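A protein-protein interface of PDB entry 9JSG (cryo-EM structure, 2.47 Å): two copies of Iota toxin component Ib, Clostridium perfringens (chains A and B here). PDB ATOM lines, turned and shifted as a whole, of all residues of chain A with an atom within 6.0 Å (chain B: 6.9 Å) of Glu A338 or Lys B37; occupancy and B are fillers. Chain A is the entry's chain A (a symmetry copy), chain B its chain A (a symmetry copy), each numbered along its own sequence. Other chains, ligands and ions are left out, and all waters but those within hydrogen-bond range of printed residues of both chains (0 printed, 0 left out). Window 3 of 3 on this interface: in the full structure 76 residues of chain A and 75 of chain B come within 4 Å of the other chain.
N of Asp B38 is in hydrogen-bond range of OE1 of Glu A338, at 2.8 Å.
O of Pro A337 sits at hydrogen-bond distance from NZ of Lys A340 (3.3 Å). N of Glu A338 sits close to OD1 of Asn A336 (3.3 Å). O of Phe B48 lies within hydrogen-bond range of N of Tyr B53. The backbone NH (N) of Leu A61 sits close to the side-chain hydroxyl (OG) of Ser A59, at 3.4 Å.
Leu A61 touches Asp B38 (CD1 to OD1, 3.9 Å). OG of Ser B39 touches CD2 of Leu A61 (3.9 Å). O of Gln B51 touches CG of Pro A337 (3.6 Å). Pro A337 touches Tyr B53. CG of Glu A338 touches O of Ile B36, at 3.5 Å. OE2 of Glu A338 touches CA of Lys B37, 3.5 Å away. Tyr B53 touches Glu A338.
Of the printed residues of chain A, Lys B37 touches Glu A338. Of the printed residues of chain A, Asp B38 touches Leu A61 (3.9 Å) and Glu A338 (2.8 Å). Printed residues of chain A within 4 Å of Gln B51: Pro A337. Thr B35 touches none of the printed residues of chain A. The nearest printed residue of chain A that does not touch Lys B37 is Leu A61 (6.0 Å).
Of the 8 printed residues of chain A, 3 touch a printed residue of chain B. Printed residues of chain A that touch a printed residue of chain B: Leu A61, Pro A337 and Glu A338. Hydrophobic or aromatic side chains of chain A within 4 Å of the printed part of chain B: Leu A61 and Pro A337. Among the printed residues, 8 pairs touch across the chains.
No position is printed for both chains. Of the 8 pairs that touch across the chains among the printed residues, none has its exchanged pair printed and touching as well.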
ATOM      1  N   SER A  59     -19.423 -19.893 -14.839  1.00  0.00           N
ATOM      2  CA  SER A  59     -19.122 -19.731 -13.423  1.00  0.00           C
ATOM      3  C   SER A  59     -19.991 -18.627 -12.836  1.00  0.00           C
ATOM      4  O   SER A  59     -20.055 -17.520 -13.381  1.00  0.00           O
ATOM      5  CB  SER A  59     -17.642 -19.406 -13.221  1.00  0.00           C
ATOM      6  OG  SER A  59     -17.351 -19.179 -11.856  1.00  0.00           O
ATOM      7  N   LEU A  61     -19.410 -17.201 -10.016  1.00  0.00           N
ATOM      8  CA  LEU A  61     -18.557 -16.289  -9.267  1.00  0.00           C
ATOM      9  C   LEU A  61     -17.680 -15.424 -10.161  1.00  0.00           C
ATOM     10  O   LEU A  61     -16.977 -14.548  -9.647  1.00  0.00           O
ATOM     11  CB  LEU A  61     -17.668 -17.073  -8.293  1.00  0.00           C
ATOM     12  CG  LEU A  61     -18.327 -17.553  -6.998  1.00  0.00           C
ATOM     13  CD1 LEU A  61     -17.342 -18.348  -6.157  1.00  0.00           C
ATOM     14  CD2 LEU A  61     -18.884 -16.378  -6.208  1.00  0.00           C
ATOM     15  N   LYS A 332     -10.850 -25.037 -15.114  1.00  0.00           N
ATOM     16  CA  LYS A 332     -10.724 -24.592 -13.736  1.00  0.00           C
ATOM     17  C   LYS A 332      -9.320 -24.860 -13.199  1.00  0.00           C
ATOM     18  O   LYS A 332      -8.560 -25.668 -13.741  1.00  0.00           O
ATOM     19  CB  LYS A 332     -11.758 -25.280 -12.844  1.00  0.00           C
ATOM     20  CG  LYS A 332     -11.413 -26.704 -12.455  1.00  0.00           C
ATOM     21  CD  LYS A 332     -12.121 -27.093 -11.163  1.00  0.00           C
ATOM     22  CE  LYS A 332     -11.904 -26.071 -10.061  1.00  0.00           C
ATOM     23  NZ  LYS A 332     -11.978 -26.688  -8.708  1.00  0.00           N
ATOM     24  N   ASN A 336      -7.910 -24.852  -6.504  1.00  0.00           N
ATOM     25  CA  ASN A 336      -8.704 -23.761  -5.943  1.00  0.00           C
ATOM     26  C   ASN A 336     -10.119 -24.235  -5.635  1.00  0.00           C
ATOM     27  O   ASN A 336     -10.841 -24.633  -6.556  1.00  0.00           O
ATOM     28  CB  ASN A 336      -8.746 -22.585  -6.907  1.00  0.00           C
ATOM     29  CG  ASN A 336      -9.140 -21.287  -6.230  1.00  0.00           C
ATOM     30  OD1 ASN A 336      -9.471 -21.268  -5.044  1.00  0.00           O
ATOM     31  ND2 ASN A 336      -9.103 -20.193  -6.980  1.00  0.00           N
ATOM     32  N   PRO A 337     -10.555 -24.213  -4.368  1.00  0.00           N
ATOM     33  CA  PRO A 337     -11.951 -24.577  -4.072  1.00  0.00           C
ATOM     34  C   PRO A 337     -12.961 -23.534  -4.520  1.00  0.00           C
ATOM     35  O   PRO A 337     -14.141 -23.873  -4.677  1.00  0.00           O
ATOM     36  CB  PRO A 337     -11.978 -24.719  -2.540  1.00  0.00           C
ATOM     37  CG  PRO A 337     -10.666 -24.260  -2.039  1.00  0.00           C
ATOM     38  CD  PRO A 337      -9.714 -24.102  -3.168  1.00  0.00           C
ATOM     39  N   GLU A 338     -12.542 -22.290  -4.730  1.00  0.00           N
ATOM     40  CA  GLU A 338     -13.447 -21.208  -5.093  1.00  0.00           C
ATOM     41  C   GLU A 338     -13.586 -21.024  -6.597  1.00  0.00           C
ATOM     42  O   GLU A 338     -14.317 -20.128  -7.029  1.00  0.00           O
ATOM     43  CB  GLU A 338     -12.978 -19.893  -4.459  1.00  0.00           C
ATOM     44  CG  GLU A 338     -13.253 -19.791  -2.969  1.00  0.00           C
ATOM     45  CD  GLU A 338     -14.735 -19.764  -2.651  1.00  0.00           C
ATOM     46  OE1 GLU A 338     -15.434 -18.861  -3.156  1.00  0.00           O
ATOM     47  OE2 GLU A 338     -15.200 -20.642  -1.897  1.00  0.00           O
ATOM     48  N   ASP A 339     -12.912 -21.840  -7.402  1.00  0.00           N
ATOM     49  CA  ASP A 339     -13.035 -21.745  -8.851  1.00  0.00           C
ATOM     50  C   ASP A 339     -14.232 -22.573  -9.300  1.00  0.00           C
ATOM     51  O   ASP A 339     -14.288 -23.781  -9.045  1.00  0.00           O
ATOM     52  CB  ASP A 339     -11.755 -22.222  -9.530  1.00  0.00           C
ATOM     53  CG  ASP A 339     -11.647 -21.746 -10.965  1.00  0.00           C
ATOM     54  OD1 ASP A 339     -12.256 -22.375 -11.851  1.00  0.00           O
ATOM     55  OD2 ASP A 339     -10.950 -20.737 -11.206  1.00  0.00           O
ATOM     56  N   LYS A 340     -15.187 -21.929  -9.968  1.00  0.00           N
ATOM     57  CA  LYS A 340     -16.441 -22.561 -10.357  1.00  0.00           C
ATOM     58  C   LYS A 340     -16.547 -22.756 -11.869  1.00  0.00           C
ATOM     59  O   LYS A 340     -17.651 -22.776 -12.420  1.00  0.00           O
ATOM     60  CB  LYS A 340     -17.628 -21.750  -9.843  1.00  0.00           C
ATOM     61  CG  LYS A 340     -17.534 -21.384  -8.372  1.00  0.00           C
ATOM     62  CD  LYS A 340     -17.588 -22.618  -7.490  1.00  0.00           C
ATOM     63  CE  LYS A 340     -17.360 -22.265  -6.030  1.00  0.00           C
ATOM     64  NZ  LYS A 340     -17.366 -23.472  -5.161  1.00  0.00           N
ATOM     65  N   THR B  35     -10.667 -16.506   5.730  1.00  0.00           N
ATOM     66  CA  THR B  35     -10.660 -17.079   4.391  1.00  0.00           C
ATOM     67  C   THR B  35     -11.755 -16.420   3.569  1.00  0.00           C
ATOM     68  O   THR B  35     -12.552 -15.630   4.081  1.00  0.00           O
ATOM     69  CB  THR B  35     -10.823 -18.604   4.427  1.00  0.00           C
ATOM     70  OG1 THR B  35     -10.272 -19.177   3.234  1.00  0.00           O
ATOM     71  CG2 THR B  35     -12.287 -18.993   4.542  1.00  0.00           C
ATOM     72  N   ILE B  36     -11.776 -16.729   2.276  1.00  0.00           N
ATOM     73  CA  ILE B  36     -12.741 -16.156   1.343  1.00  0.00           C
ATOM     74  C   ILE B  36     -13.603 -17.283   0.794  1.00  0.00           C
ATOM     75  O   ILE B  36     -13.085 -18.238   0.201  1.00  0.00           O
ATOM     76  CB  ILE B  36     -12.050 -15.390   0.204  1.00  0.00           C
ATOM     77  CG1 ILE B  36     -11.015 -14.412   0.767  1.00  0.00           C
ATOM     78  CG2 ILE B  36     -13.082 -14.671  -0.655  1.00  0.00           C
ATOM     79  CD1 ILE B  36     -11.584 -13.060   1.146  1.00  0.00           C
ATOM     80  N   LYS B  37     -14.915 -17.170   0.990  1.00  0.00           N
ATOM     81  CA  LYS B  37     -15.887 -18.106   0.437  1.00  0.00           C
ATOM     82  C   LYS B  37     -16.992 -17.306  -0.230  1.00  0.00           C
ATOM     83  O   LYS B  37     -17.573 -16.411   0.393  1.00  0.00           O
ATOM     84  CB  LYS B  37     -16.462 -19.019   1.524  1.00  0.00           C
ATOM     85  CG  LYS B  37     -15.458 -19.995   2.115  1.00  0.00           C
ATOM     86  CD  LYS B  37     -16.099 -20.865   3.183  1.00  0.00           C
ATOM     87  CE  LYS B  37     -15.127 -21.913   3.697  1.00  0.00           C
ATOM     88  NZ  LYS B  37     -15.799 -23.221   3.936  1.00  0.00           N
ATOM     89  N   ASP B  38     -17.280 -17.628  -1.494  1.00  0.00           N
ATOM     90  CA  ASP B  38     -18.311 -16.936  -2.272  1.00  0.00           C
ATOM     91  C   ASP B  38     -18.083 -15.427  -2.275  1.00  0.00           C
ATOM     92  O   ASP B  38     -19.020 -14.636  -2.140  1.00  0.00           O
ATOM     93  CB  ASP B  38     -19.708 -17.280  -1.758  1.00  0.00           C
ATOM     94  CG  ASP B  38     -20.210 -18.615  -2.278  1.00  0.00           C
ATOM     95  OD1 ASP B  38     -19.474 -19.269  -3.045  1.00  0.00           O
ATOM     96  OD2 ASP B  38     -21.339 -19.007  -1.919  1.00  0.00           O
ATOM     97  N   SER B  39     -16.817 -15.028  -2.422  1.00  0.00           N
ATOM     98  CA  SER B  39     -16.410 -13.622  -2.434  1.00  0.00           C
ATOM     99  C   SER B  39     -16.793 -12.906  -1.142  1.00  0.00           C
ATOM    100  O   SER B  39     -17.069 -11.703  -1.144  1.00  0.00           O
ATOM    101  CB  SER B  39     -16.988 -12.884  -3.645  1.00  0.00           C
ATOM    102  OG  SER B  39     -16.578 -13.494  -4.858  1.00  0.00           O
ATOM    103  N   ILE B  40     -16.814 -13.636  -0.028  1.00  0.00           N
ATOM    104  CA  ILE B  40     -17.120 -13.076   1.283  1.00  0.00           C
ATOM    105  C   ILE B  40     -16.046 -13.531   2.259  1.00  0.00           C
ATOM    106  O   ILE B  40     -15.709 -14.720   2.306  1.00  0.00           O
ATOM    107  CB  ILE B  40     -18.517 -13.499   1.778  1.00  0.00           C
ATOM    108  CG1 ILE B  40     -19.603 -12.977   0.833  1.00  0.00           C
ATOM    109  CG2 ILE B  40     -18.754 -13.015   3.203  1.00  0.00           C
ATOM    110  CD1 ILE B  40     -20.015 -11.543   1.099  1.00  0.00           C
ATOM    111  N   ALA B  41     -15.502 -12.591   3.028  1.00  0.00           N
ATOM    112  CA  ALA B  41     -14.498 -12.918   4.029  1.00  0.00           C
ATOM    113  C   ALA B  41     -15.170 -13.484   5.273  1.00  0.00           C
ATOM    114  O   ALA B  41     -16.056 -12.849   5.854  1.00  0.00           O
ATOM    115  CB  ALA B  41     -13.673 -11.681   4.385  1.00  0.00           C
ATOM    116  N   VAL B  42     -14.746 -14.681   5.681  1.00  0.00           N
ATOM    117  CA  VAL B  42     -15.314 -15.363   6.834  1.00  0.00           C
ATOM    118  C   VAL B  42     -14.192 -15.776   7.776  1.00  0.00           C
ATOM    119  O   VAL B  42     -13.025 -15.899   7.389  1.00  0.00           O
ATOM    120  CB  VAL B  42     -16.166 -16.593   6.439  1.00  0.00           C
ATOM    121  CG1 VAL B  42     -17.112 -16.253   5.296  1.00  0.00           C
ATOM    122  CG2 VAL B  42     -15.277 -17.768   6.074  1.00  0.00           C
ATOM    123  N   LYS B  43     -14.570 -15.982   9.038  1.00  0.00           N
ATOM    124  CA  LYS B  43     -13.614 -16.348  10.074  1.00  0.00           C
ATOM    125  C   LYS B  43     -13.024 -17.727   9.797  1.00  0.00           C
ATOM    126  O   LYS B  43     -13.726 -18.650   9.376  1.00  0.00           O
ATOM    127  CB  LYS B  43     -14.300 -16.324  11.441  1.00  0.00           C
ATOM    128  CG  LYS B  43     -13.443 -16.802  12.601  1.00  0.00           C
ATOM    129  CD  LYS B  43     -13.767 -16.028  13.869  1.00  0.00           C
ATOM    130  CE  LYS B  43     -14.243 -16.952  14.979  1.00  0.00           C
ATOM    131  NZ  LYS B  43     -13.126 -17.746  15.564  1.00  0.00           N
ATOM    132  N   PHE B  48     -11.728 -26.134   7.439  1.00  0.00           N
ATOM    133  CA  PHE B  48     -11.654 -25.573   6.095  1.00  0.00           C
ATOM    134  C   PHE B  48     -10.382 -25.986   5.373  1.00  0.00           C
ATOM    135  O   PHE B  48     -10.403 -26.145   4.146  1.00  0.00           O
ATOM    136  CB  PHE B  48     -11.730 -24.045   6.148  1.00  0.00           C
ATOM    137  CG  PHE B  48     -13.050 -23.514   6.623  1.00  0.00           C
ATOM    138  CD1 PHE B  48     -14.152 -24.345   6.741  1.00  0.00           C
ATOM    139  CD2 PHE B  48     -13.191 -22.175   6.947  1.00  0.00           C
ATOM    140  CE1 PHE B  48     -15.364 -23.852   7.176  1.00  0.00           C
ATOM    141  CE2 PHE B  48     -14.402 -21.677   7.382  1.00  0.00           C
ATOM    142  CZ  PHE B  48     -15.490 -22.517   7.497  1.00  0.00           C
ATOM    143  N   GLN B  51     -10.660 -28.812   2.986  1.00  0.00           N
ATOM    144  CA  GLN B  51     -11.312 -28.576   1.706  1.00  0.00           C
ATOM    145  C   GLN B  51     -10.444 -27.788   0.733  1.00  0.00           C
ATOM    146  O   GLN B  51     -10.901 -27.487  -0.375  1.00  0.00           O
ATOM    147  CB  GLN B  51     -12.642 -27.845   1.910  1.00  0.00           C
ATOM    148  CG  GLN B  51     -13.392 -28.241   3.168  1.00  0.00           C
ATOM    149  CD  GLN B  51     -14.500 -27.264   3.505  1.00  0.00           C
ATOM    150  OE1 GLN B  51     -14.558 -26.730   4.611  1.00  0.00           O
ATOM    151  NE2 GLN B  51     -15.389 -27.029   2.548  1.00  0.00           N
ATOM    152  N   TYR B  53      -8.889 -24.716   1.500  1.00  0.00           N
ATOM    153  CA  TYR B  53      -8.822 -23.294   1.796  1.00  0.00           C
ATOM    154  C   TYR B  53      -7.523 -22.956   2.520  1.00  0.00           C
ATOM    155  O   TYR B  53      -6.935 -23.794   3.210  1.00  0.00           O
ATOM    156  CB  TYR B  53     -10.024 -22.867   2.640  1.00  0.00           C
ATOM    157  CG  TYR B  53     -11.331 -22.889   1.882  1.00  0.00           C
ATOM    158  CD1 TYR B  53     -11.714 -21.811   1.093  1.00  0.00           C
ATOM    159  CD2 TYR B  53     -12.179 -23.985   1.952  1.00  0.00           C
ATOM    160  CE1 TYR B  53     -12.907 -21.827   0.399  1.00  0.00           C
ATOM    161  CE2 TYR B  53     -13.374 -24.009   1.261  1.00  0.00           C
ATOM    162  CZ  TYR B  53     -13.733 -22.928   0.485  1.00  0.00           C
ATOM    163  N   SER B  77      -9.244 -12.711  -2.294  1.00  0.00           N
ATOM    164  CA  SER B  77     -10.423 -13.199  -2.996  1.00  0.00           C
ATOM    165  C   SER B  77     -10.123 -13.670  -4.413  1.00  0.00           C
ATOM    166  O   SER B  77     -10.899 -14.458  -4.964  1.00  0.00           O
ATOM    167  CB  SER B  77     -11.498 -12.111  -3.037  1.00  0.00           C
ATOM    168  OG  SER B  77     -10.998 -10.926  -3.636  1.00  0.00           O
